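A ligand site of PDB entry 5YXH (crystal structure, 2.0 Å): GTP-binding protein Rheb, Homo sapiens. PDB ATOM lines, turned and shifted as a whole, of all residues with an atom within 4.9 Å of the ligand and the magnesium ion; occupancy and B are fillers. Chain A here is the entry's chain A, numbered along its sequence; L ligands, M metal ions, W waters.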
ATOM      1  N   TYR A  14     -10.636 -20.878 -15.983  1.00  0.00           N
ATOM      2  CA  TYR A  14     -11.844 -20.476 -16.694  1.00  0.00           C
ATOM      3  C   TYR A  14     -12.712 -19.595 -15.794  1.00  0.00           C
ATOM      4  O   TYR A  14     -12.574 -19.641 -14.577  1.00  0.00           O
ATOM      5  CB  TYR A  14     -12.605 -21.741 -17.120  1.00  0.00           C
ATOM      6  CG  TYR A  14     -13.794 -21.558 -18.029  1.00  0.00           C
ATOM      7  CD1 TYR A  14     -13.699 -20.843 -19.219  1.00  0.00           C
ATOM      8  CD2 TYR A  14     -15.019 -22.160 -17.728  1.00  0.00           C
ATOM      9  CE1 TYR A  14     -14.784 -20.708 -20.069  1.00  0.00           C
ATOM     10  CE2 TYR A  14     -16.107 -22.020 -18.564  1.00  0.00           C
ATOM     11  CZ  TYR A  14     -15.994 -21.293 -19.732  1.00  0.00           C
ATOM     12  OH  TYR A  14     -17.086 -21.172 -20.563  1.00  0.00           O
ATOM     13  N   ARG A  15     -13.558 -18.772 -16.394  1.00  0.00           N
ATOM     14  CA  ARG A  15     -14.421 -17.874 -15.621  1.00  0.00           C
ATOM     15  C   ARG A  15     -15.430 -18.657 -14.785  1.00  0.00           C
ATOM     16  O   ARG A  15     -15.873 -19.733 -15.169  1.00  0.00           O
ATOM     17  CB  ARG A  15     -15.183 -16.904 -16.539  1.00  0.00           C
ATOM     18  CG  ARG A  15     -15.786 -17.567 -17.757  1.00  0.00           C
ATOM     19  CD  ARG A  15     -16.989 -16.847 -18.313  1.00  0.00           C
ATOM     20  NE  ARG A  15     -17.424 -17.514 -19.534  1.00  0.00           N
ATOM     21  CZ  ARG A  15     -16.836 -17.379 -20.722  1.00  0.00           C
ATOM     22  NH1 ARG A  15     -15.786 -16.575 -20.890  1.00  0.00           N
ATOM     23  NH2 ARG A  15     -17.310 -18.050 -21.760  1.00  0.00           N
ATOM     24  N   SER A  16     -15.772 -18.090 -13.630  1.00  0.00           N
ATOM     25  CA  SER A  16     -16.719 -18.681 -12.670  1.00  0.00           C
ATOM     26  C   SER A  16     -16.307 -20.029 -12.034  1.00  0.00           C
ATOM     27  O   SER A  16     -17.155 -20.755 -11.517  1.00  0.00           O
ATOM     28  CB  SER A  16     -18.145 -18.742 -13.268  1.00  0.00           C
ATOM     29  OG  SER A  16     -18.160 -19.326 -14.558  1.00  0.00           O
ATOM     30  N   VAL A  17     -15.007 -20.354 -12.033  1.00  0.00           N
ATOM     31  CA  VAL A  17     -14.515 -21.543 -11.303  1.00  0.00           C
ATOM     32  C   VAL A  17     -14.388 -21.276  -9.811  1.00  0.00           C
ATOM     33  O   VAL A  17     -14.425 -22.206  -9.001  1.00  0.00           O
ATOM     34  CB  VAL A  17     -13.159 -22.064 -11.841  1.00  0.00           C
ATOM     35  CG1 VAL A  17     -13.291 -22.527 -13.278  1.00  0.00           C
ATOM     36  CG2 VAL A  17     -12.051 -21.025 -11.695  1.00  0.00           C
ATOM     37  N   GLY A  18     -14.227 -20.000  -9.451  1.00  0.00           N
ATOM     38  CA  GLY A  18     -14.103 -19.598  -8.049  1.00  0.00           C
ATOM     39  C   GLY A  18     -12.740 -19.039  -7.687  1.00  0.00           C
ATOM     40  O   GLY A  18     -12.353 -19.065  -6.515  1.00  0.00           O
ATOM     41  N   LYS A  19     -12.020 -18.519  -8.693  1.00  0.00           N
ATOM     42  CA  LYS A  19     -10.719 -17.898  -8.492  1.00  0.00           C
ATOM     43  C   LYS A  19     -10.822 -16.764  -7.480  1.00  0.00           C
ATOM     44  O   LYS A  19     -10.053 -16.707  -6.523  1.00  0.00           O
ATOM     45  CB  LYS A  19     -10.187 -17.306  -9.795  1.00  0.00           C
ATOM     46  CG  LYS A  19      -9.794 -18.304 -10.860  1.00  0.00           C
ATOM     47  CD  LYS A  19      -9.168 -17.597 -12.060  1.00  0.00           C
ATOM     48  CE  LYS A  19     -10.128 -16.637 -12.750  1.00  0.00           C
ATOM     49  NZ  LYS A  19     -11.357 -17.311 -13.268  1.00  0.00           N
ATOM     50  N   SER A  20     -11.766 -15.852  -7.728  1.00  0.00           N
ATOM     51  CA  SER A  20     -11.981 -14.728  -6.834  1.00  0.00           C
ATOM     52  C   SER A  20     -12.473 -15.220  -5.487  1.00  0.00           C
ATOM     53  O   SER A  20     -11.881 -14.872  -4.457  1.00  0.00           O
ATOM     54  CB  SER A  20     -12.959 -13.711  -7.448  1.00  0.00           C
ATOM     55  OG  SER A  20     -12.384 -13.053  -8.560  1.00  0.00           O
ATOM     56  N   SER A  21     -13.529 -16.037  -5.483  1.00  0.00           N
ATOM     57  CA  SER A  21     -14.089 -16.552  -4.234  1.00  0.00           C
ATOM     58  C   SER A  21     -13.047 -17.210  -3.352  1.00  0.00           C
ATOM     59  O   SER A  21     -13.022 -16.982  -2.148  1.00  0.00           O
ATOM     60  CB  SER A  21     -15.246 -17.531  -4.501  1.00  0.00           C
ATOM     61  OG  SER A  21     -16.414 -16.846  -4.894  1.00  0.00           O
ATOM     62  N   PHE A  31     -16.807 -15.830   2.543  1.00  0.00           N
ATOM     63  CA  PHE A  31     -17.240 -16.348   1.251  1.00  0.00           C
ATOM     64  C   PHE A  31     -18.152 -15.339   0.547  1.00  0.00           C
ATOM     65  O   PHE A  31     -19.211 -14.980   1.070  1.00  0.00           O
ATOM     66  CB  PHE A  31     -17.939 -17.694   1.447  1.00  0.00           C
ATOM     67  CG  PHE A  31     -18.589 -18.234   0.217  1.00  0.00           C
ATOM     68  CD1 PHE A  31     -17.814 -18.640  -0.871  1.00  0.00           C
ATOM     69  CD2 PHE A  31     -19.959 -18.325   0.118  1.00  0.00           C
ATOM     70  CE1 PHE A  31     -18.410 -19.127  -2.024  1.00  0.00           C
ATOM     71  CE2 PHE A  31     -20.565 -18.819  -1.027  1.00  0.00           C
ATOM     72  CZ  PHE A  31     -19.788 -19.219  -2.094  1.00  0.00           C
ATOM     73  N   VAL A  32     -17.751 -14.912  -0.646  1.00  0.00           N
ATOM     74  CA  VAL A  32     -18.465 -13.869  -1.388  1.00  0.00           C
ATOM     75  C   VAL A  32     -19.285 -14.450  -2.549  1.00  0.00           C
ATOM     76  O   VAL A  32     -18.834 -15.365  -3.243  1.00  0.00           O
ATOM     77  CB  VAL A  32     -17.484 -12.795  -1.923  1.00  0.00           C
ATOM     78  CG1 VAL A  32     -16.736 -13.290  -3.162  1.00  0.00           C
ATOM     79  CG2 VAL A  32     -18.205 -11.490  -2.230  1.00  0.00           C
ATOM     80  N   ASP A  33     -20.491 -13.919  -2.726  1.00  0.00           N
ATOM     81  CA  ASP A  33     -21.336 -14.249  -3.883  1.00  0.00           C
ATOM     82  C   ASP A  33     -21.173 -13.159  -4.931  1.00  0.00           C
ATOM     83  O   ASP A  33     -20.843 -13.436  -6.084  1.00  0.00           O
ATOM     84  CB  ASP A  33     -22.812 -14.332  -3.469  1.00  0.00           C
ATOM     85  CG  ASP A  33     -23.098 -15.489  -2.522  1.00  0.00           C
ATOM     86  OD1 ASP A  33     -22.409 -16.529  -2.619  1.00  0.00           O
ATOM     87  OD2 ASP A  33     -24.015 -15.348  -1.688  1.00  0.00           O
ATOM     88  N   TYR A  35     -19.152 -10.867  -6.543  1.00  0.00           N
ATOM     89  CA  TYR A  35     -17.875 -10.331  -7.001  1.00  0.00           C
ATOM     90  C   TYR A  35     -17.818 -10.363  -8.539  1.00  0.00           C
ATOM     91  O   TYR A  35     -18.199 -11.359  -9.157  1.00  0.00           O
ATOM     92  CB  TYR A  35     -16.697 -11.096  -6.398  1.00  0.00           C
ATOM     93  CG  TYR A  35     -15.421 -10.276  -6.342  1.00  0.00           C
ATOM     94  CD1 TYR A  35     -15.173  -9.393  -5.283  1.00  0.00           C
ATOM     95  CD2 TYR A  35     -14.460 -10.372  -7.357  1.00  0.00           C
ATOM     96  CE1 TYR A  35     -14.010  -8.646  -5.227  1.00  0.00           C
ATOM     97  CE2 TYR A  35     -13.297  -9.624  -7.301  1.00  0.00           C
ATOM     98  CZ  TYR A  35     -13.072  -8.759  -6.248  1.00  0.00           C
ATOM     99  OH  TYR A  35     -11.908  -8.025  -6.203  1.00  0.00           O
ATOM    100  N   ASP A  36     -17.347  -9.265  -9.141  1.00  0.00           N
ATOM    101  CA  ASP A  36     -17.420  -9.065 -10.592  1.00  0.00           C
ATOM    102  C   ASP A  36     -16.344  -9.831 -11.380  1.00  0.00           C
ATOM    103  O   ASP A  36     -15.147  -9.634 -11.146  1.00  0.00           O
ATOM    104  CB  ASP A  36     -17.388  -7.572 -10.949  1.00  0.00           C
ATOM    105  CG  ASP A  36     -16.205  -6.838 -10.363  1.00  0.00           C
ATOM    106  OD1 ASP A  36     -15.771  -7.207  -9.245  1.00  0.00           O
ATOM    107  OD2 ASP A  36     -15.708  -5.881 -10.996  1.00  0.00           O
ATOM    108  N   PRO A  37     -16.753 -10.711 -12.321  1.00  0.00           N
ATOM    109  CA  PRO A  37     -15.812 -11.556 -13.081  1.00  0.00           C
ATOM    110  C   PRO A  37     -15.008 -10.896 -14.199  1.00  0.00           C
ATOM    111  O   PRO A  37     -14.399 -11.610 -15.001  1.00  0.00           O
ATOM    112  CB  PRO A  37     -16.721 -12.630 -13.691  1.00  0.00           C
ATOM    113  CG  PRO A  37     -18.013 -12.554 -12.950  1.00  0.00           C
ATOM    114  CD  PRO A  37     -18.146 -11.127 -12.539  1.00  0.00           C
ATOM    115  N   ASP A  60      -5.249 -12.390  -8.845  1.00  0.00           N
ATOM    116  CA  ASP A  60      -6.508 -13.016  -9.217  1.00  0.00           C
ATOM    117  C   ASP A  60      -6.924 -12.526 -10.606  1.00  0.00           C
ATOM    118  O   ASP A  60      -7.564 -11.485 -10.734  1.00  0.00           O
ATOM    119  CB  ASP A  60      -7.573 -12.680  -8.181  1.00  0.00           C
ATOM    120  CG  ASP A  60      -8.948 -13.143  -8.585  1.00  0.00           C
ATOM    121  OD1 ASP A  60      -9.056 -14.134  -9.322  1.00  0.00           O
ATOM    122  OD2 ASP A  60      -9.924 -12.497  -8.146  1.00  0.00           O
ATOM    123  N   THR A  61      -6.553 -13.285 -11.631  1.00  0.00           N
ATOM    124  CA  THR A  61      -6.856 -12.910 -13.005  1.00  0.00           C
ATOM    125  C   THR A  61      -8.357 -12.901 -13.261  1.00  0.00           C
ATOM    126  O   THR A  61      -9.136 -13.514 -12.517  1.00  0.00           O
ATOM    127  CB  THR A  61      -6.167 -13.849 -14.020  1.00  0.00           C
ATOM    128  OG1 THR A  61      -6.528 -15.207 -13.766  1.00  0.00           O
ATOM    129  CG2 THR A  61      -4.656 -13.700 -13.949  1.00  0.00           C
ATOM    130  N   ALA A  62      -8.766 -12.171 -14.280  1.00  0.00           N
ATOM    131  CA  ALA A  62     -10.149 -12.152 -14.713  1.00  0.00           C
ATOM    132  C   ALA A  62     -10.594 -13.587 -15.019  1.00  0.00           C
ATOM    133  O   ALA A  62     -11.587 -14.067 -14.490  1.00  0.00           O
ATOM    134  CB  ALA A  62     -10.313 -11.269 -15.950  1.00  0.00           C
ATOM    135  N   ASN A 119     -11.848 -26.684  -7.525  1.00  0.00           N
ATOM    136  CA  ASN A 119     -12.734 -25.980  -6.588  1.00  0.00           C
ATOM    137  C   ASN A 119     -14.215 -26.384  -6.714  1.00  0.00           C
ATOM    138  O   ASN A 119     -14.607 -27.074  -7.646  1.00  0.00           O
ATOM    139  CB  ASN A 119     -12.594 -24.472  -6.814  1.00  0.00           C
ATOM    140  CG  ASN A 119     -13.160 -23.653  -5.682  1.00  0.00           C
ATOM    141  OD1 ASN A 119     -13.000 -23.991  -4.509  1.00  0.00           O
ATOM    142  ND2 ASN A 119     -13.858 -22.577  -6.030  1.00  0.00           N
ATOM    143  N   LYS A 120     -15.021 -25.941  -5.743  1.00  0.00           N
ATOM    144  CA  LYS A 120     -16.469 -26.181  -5.673  1.00  0.00           C
ATOM    145  C   LYS A 120     -16.771 -27.610  -5.255  1.00  0.00           C
ATOM    146  O   LYS A 120     -17.832 -28.148  -5.578  1.00  0.00           O
ATOM    147  CB  LYS A 120     -17.181 -25.855  -7.000  1.00  0.00           C
ATOM    148  CG  LYS A 120     -16.864 -24.480  -7.564  1.00  0.00           C
ATOM    149  CD  LYS A 120     -18.042 -23.947  -8.350  1.00  0.00           C
ATOM    150  CE  LYS A 120     -17.744 -22.595  -8.971  1.00  0.00           C
ATOM    151  NZ  LYS A 120     -18.827 -22.164  -9.901  1.00  0.00           N
ATOM    152  N   LYS A 121     -15.857 -28.208  -4.480  1.00  0.00           N
ATOM    153  CA  LYS A 121     -16.007 -29.585  -4.025  1.00  0.00           C
ATOM    154  C   LYS A 121     -17.212 -29.785  -3.108  1.00  0.00           C
ATOM    155  O   LYS A 121     -17.675 -30.903  -2.908  1.00  0.00           O
ATOM    156  CB  LYS A 121     -14.745 -30.058  -3.302  1.00  0.00           C
ATOM    157  CG  LYS A 121     -14.611 -29.518  -1.890  1.00  0.00           C
ATOM    158  CD  LYS A 121     -13.276 -29.883  -1.256  1.00  0.00           C
ATOM    159  CE  LYS A 121     -13.461 -30.848  -0.079  1.00  0.00           C
ATOM    160  NZ  LYS A 121     -14.098 -30.191   1.100  1.00  0.00           N
ATOM    161  N   ASP A 122     -17.688 -28.689  -2.509  1.00  0.00           N
ATOM    162  CA  ASP A 122     -18.859 -28.728  -1.638  1.00  0.00           C
ATOM    163  C   ASP A 122     -20.163 -29.052  -2.398  1.00  0.00           C
ATOM    164  O   ASP A 122     -21.134 -29.481  -1.783  1.00  0.00           O
ATOM    165  CB  ASP A 122     -19.007 -27.412  -0.876  1.00  0.00           C
ATOM    166  CG  ASP A 122     -19.170 -26.218  -1.798  1.00  0.00           C
ATOM    167  OD1 ASP A 122     -18.139 -25.702  -2.285  1.00  0.00           O
ATOM    168  OD2 ASP A 122     -20.314 -25.795  -2.048  1.00  0.00           O
ATOM    169  N   LEU A 123     -20.167 -28.850  -3.714  1.00  0.00           N
ATOM    170  CA  LEU A 123     -21.376 -29.047  -4.519  1.00  0.00           C
ATOM    171  C   LEU A 123     -21.551 -30.493  -5.001  1.00  0.00           C
ATOM    172  O   LEU A 123     -21.489 -30.782  -6.205  1.00  0.00           O
ATOM    173  CB  LEU A 123     -21.393 -28.062  -5.698  1.00  0.00           C
ATOM    174  CG  LEU A 123     -21.621 -26.592  -5.352  1.00  0.00           C
ATOM    175  CD1 LEU A 123     -21.563 -25.717  -6.602  1.00  0.00           C
ATOM    176  CD2 LEU A 123     -22.953 -26.418  -4.636  1.00  0.00           C
ATOM    177  N   SER A 148     -10.877 -27.983  -3.299  1.00  0.00           N
ATOM    178  CA  SER A 148     -11.169 -26.901  -2.385  1.00  0.00           C
ATOM    179  C   SER A 148     -12.632 -26.500  -2.459  1.00  0.00           C
ATOM    180  O   SER A 148     -13.342 -26.823  -3.416  1.00  0.00           O
ATOM    181  CB  SER A 148     -10.317 -25.684  -2.735  1.00  0.00           C
ATOM    182  OG  SER A 148     -10.610 -25.205  -4.034  1.00  0.00           O
ATOM    183  N   SER A 149     -13.078 -25.813  -1.410  1.00  0.00           N
ATOM    184  CA  SER A 149     -14.351 -25.110  -1.399  1.00  0.00           C
ATOM    185  C   SER A 149     -14.083 -23.710  -0.898  1.00  0.00           C
ATOM    186  O   SER A 149     -13.569 -23.526   0.208  1.00  0.00           O
ATOM    187  CB  SER A 149     -15.362 -25.791  -0.468  1.00  0.00           C
ATOM    188  OG  SER A 149     -16.534 -24.992  -0.309  1.00  0.00           O
ATOM    189  N   ALA A 150     -14.418 -22.715  -1.714  1.00  0.00           N
ATOM    190  CA  ALA A 150     -14.354 -21.310  -1.309  1.00  0.00           C
ATOM    191  C   ALA A 150     -15.240 -20.992  -0.087  1.00  0.00           C
ATOM    192  O   ALA A 150     -15.050 -19.950   0.553  1.00  0.00           O
ATOM    193  CB  ALA A 150     -14.717 -20.396  -2.469  1.00  0.00           C
ATOM    194  N   LYS A 151     -16.202 -21.871   0.214  1.00  0.00           N
ATOM    195  CA  LYS A 151     -17.011 -21.779   1.443  1.00  0.00           C
ATOM    196  C   LYS A 151     -16.303 -22.262   2.699  1.00  0.00           C
ATOM    197  O   LYS A 151     -16.799 -22.048   3.801  1.00  0.00           O
ATOM    198  CB  LYS A 151     -18.291 -22.637   1.323  1.00  0.00           C
ATOM    199  CG  LYS A 151     -19.267 -22.216   0.252  1.00  0.00           C
ATOM    200  CD  LYS A 151     -20.650 -22.785   0.555  1.00  0.00           C
ATOM    201  CE  LYS A 151     -21.652 -22.364  -0.499  1.00  0.00           C
ATOM    202  NZ  LYS A 151     -22.997 -22.940  -0.231  1.00  0.00           N
HETATM  203  P1  LIG L   1     -14.148 -16.511 -10.925  1.00  0.00           P
HETATM  204  O1  LIG L   1     -13.580 -15.509  -9.960  1.00  0.00           O
HETATM  205  O2  LIG L   1     -13.217 -17.638 -11.300  1.00  0.00           O
HETATM  206  O3  LIG L   1     -14.936 -15.965 -12.090  1.00  0.00           O
HETATM  207  O4  LIG L   1     -15.304 -17.193 -10.031  1.00  0.00           O
HETATM  208  P2  LIG L   1     -16.001 -16.429  -8.816  1.00  0.00           P
HETATM  209  O5  LIG L   1     -16.565 -15.115  -9.275  1.00  0.00           O
HETATM  210  O6  LIG L   1     -15.073 -16.446  -7.628  1.00  0.00           O
HETATM  211  O7  LIG L   1     -17.255 -17.373  -8.471  1.00  0.00           O
HETATM  212  C1  LIG L   1     -18.287 -17.630  -9.431  1.00  0.00           C
HETATM  213  C2  LIG L   1     -19.560 -18.065  -8.725  1.00  0.00           C
HETATM  214  O8  LIG L   1     -19.357 -19.349  -8.130  1.00  0.00           O
HETATM  215  C3  LIG L   1     -19.944 -17.132  -7.584  1.00  0.00           C
HETATM  216  O9  LIG L   1     -21.370 -17.120  -7.433  1.00  0.00           O
HETATM  217  C4  LIG L   1     -19.322 -17.778  -6.368  1.00  0.00           C
HETATM  218  O10 LIG L   1     -19.983 -17.394  -5.159  1.00  0.00           O
HETATM  219  C5  LIG L   1     -19.458 -19.254  -6.704  1.00  0.00           C
HETATM  220  N1  LIG L   1     -18.385 -20.093  -6.105  1.00  0.00           N
HETATM  221  C6  LIG L   1     -17.065 -19.930  -6.237  1.00  0.00           C
HETATM  222  N2  LIG L   1     -16.386 -20.903  -5.577  1.00  0.00           N
HETATM  223  C7  LIG L   1     -17.296 -21.717  -5.006  1.00  0.00           C
HETATM  224  C8  LIG L   1     -17.278 -22.936  -4.167  1.00  0.00           C
HETATM  225  O11 LIG L   1     -16.199 -23.474  -3.809  1.00  0.00           O
HETATM  226  N3  LIG L   1     -18.453 -23.464  -3.789  1.00  0.00           N
HETATM  227  C9  LIG L   1     -19.639 -22.928  -4.160  1.00  0.00           C
HETATM  228  N4  LIG L   1     -20.788 -23.514  -3.743  1.00  0.00           N
HETATM  229  N5  LIG L   1     -19.727 -21.812  -4.927  1.00  0.00           N
HETATM  230  C10 LIG L   1     -18.609 -21.174  -5.368  1.00  0.00           C
HETATM  231 MG    MG M   1     -13.447 -13.393 -10.439  1.00  0.00          MG
HETATM  232  O   HOH W   1     -13.476 -13.736 -12.576  1.00  0.00           O
HETATM  233  O   HOH W   2     -11.292 -13.571 -10.599  1.00  0.00           O
HETATM  234  O   HOH W   3     -12.709 -11.344 -10.667  1.00  0.00           O
HETATM  235  O   HOH W   4     -15.473 -12.801  -9.918  1.00  0.00           O
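The backbone NH (N) of Lys 19 sits at hydrogen-bond distance from an oxygen (O2) of the ligand (3.0 Å). The backbone NH (N) of Gly 18 sits at hydrogen-bond distance from an oxygen (O4) of the ligand (3.1 Å). ND2 of Asn 119 sits at hydrogen-bond distance from N2 of the ligand, at 3.1 Å. OD1 of Asp 122 lies within hydrogen-bond range of N3 of the ligand, 2.7 Å away. OG of Ser 21 sits at hydrogen-bond distance from O6 of the ligand. N of Ser 16 is in hydrogen-bond range of O3 of the ligand. N of Ser 20 lies within hydrogen-bond range of O6 of the ligand (3.4 Å). NZ of Lys 120 is in hydrogen-bond range of O8 of the ligand (3.4 Å). N of Val 17 sits at hydrogen-bond distance from O2 of the ligand (3.3 Å). An oxygen (O2) of the ligand is in salt-bridge range of the side-chain amino group (NZ) of Lys 19 (2.7 Å). The backbone NH of Lys 120 sits close to an oxygen (O11) of the ligand (3.3 Å). The backbone NH (N) of Ala 150 sits at hydrogen-bond distance from an oxygen (O11) of the ligand (2.9 Å). The backbone carbonyl oxygen of Val 32 is in hydrogen-bond range of an oxygen (O10) of the ligand (3.0 Å). The backbone NH of Ser 21 lies within hydrogen-bond range of an oxygen (O6) of the ligand.
The side-chain hydroxyl of Ser 20 lies close to the side-chain carboxylate of Asp 60 (2.6 Å). The backbone carbonyl oxygen of Ala 62 lies close to the side-chain amino group of Lys 19, 3.5 Å away. OG of Ser 21 lies within hydrogen-bond range of O of Val 32, 3.3 Å away. N of Ala 150 sits at hydrogen-bond distance from OD1 of Asn 119. N of Lys 120 sits at hydrogen-bond distance from O of Ser 148 (3.0 Å). The side-chain hydroxyl of Ser 148 lies within hydrogen-bond range of the side-chain amide oxygen of Asn 119, at 2.7 Å. The side-chain amino group (NZ) of Lys 19 is in hydrogen-bond range of the backbone carbonyl oxygen (O) of Tyr 14 (2.9 Å). The side-chain amino group (NZ) of Lys 120 is in hydrogen-bond range of the backbone carbonyl oxygen (O) of Ser 16.
Water W4 lies within hydrogen-bond range of O5 of the ligand, O of Tyr 35 and O of Asp 36. Water W2 bridges OD1 of Asp 60 (2.6 Å) and O of Thr 61 (2.9 Å). Water W1 lies within hydrogen-bond range of an oxygen (O3) of the ligand (2.7 Å), the backbone carbonyl oxygen of Ala 62 (2.7 Å) and the backbone carbonyl oxygen of Pro 37 (3.4 Å).
Water W1 binds the magnesium ion (2.2 Å). The magnesium ion is bound by water W2 (2.2 Å). O1 of the ligand binds the magnesium ion (2.2 Å). The magnesium ion is bound by water W4, 2.2 Å away. The side-chain hydroxyl (OG) of Ser 20 is bound to the magnesium ion. Water W3 binds the magnesium ion, 2.2 Å away.
Merely in contact with the ligand: Ser 149, Lys 151, Leu 123, Phe 31, Asp 33, Arg 15 and Tyr 14. Hydrophobic or aromatic side chains within 4 Å of the ligand: Val 17, Phe 31, Leu 123 and Ala 150. Within 4 Å of the ligand: Tyr 14, Arg 15, Ser 16, Val 17, Gly 18, Lys 19, Ser 20, Ser 21, Phe 31, Val 32, Asp 33, Asn 119, Lys 120, Asp 122, Leu 123, Ser 149, Ala 150 and Lys 151.
Pro 37 touches the magnesium ion.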
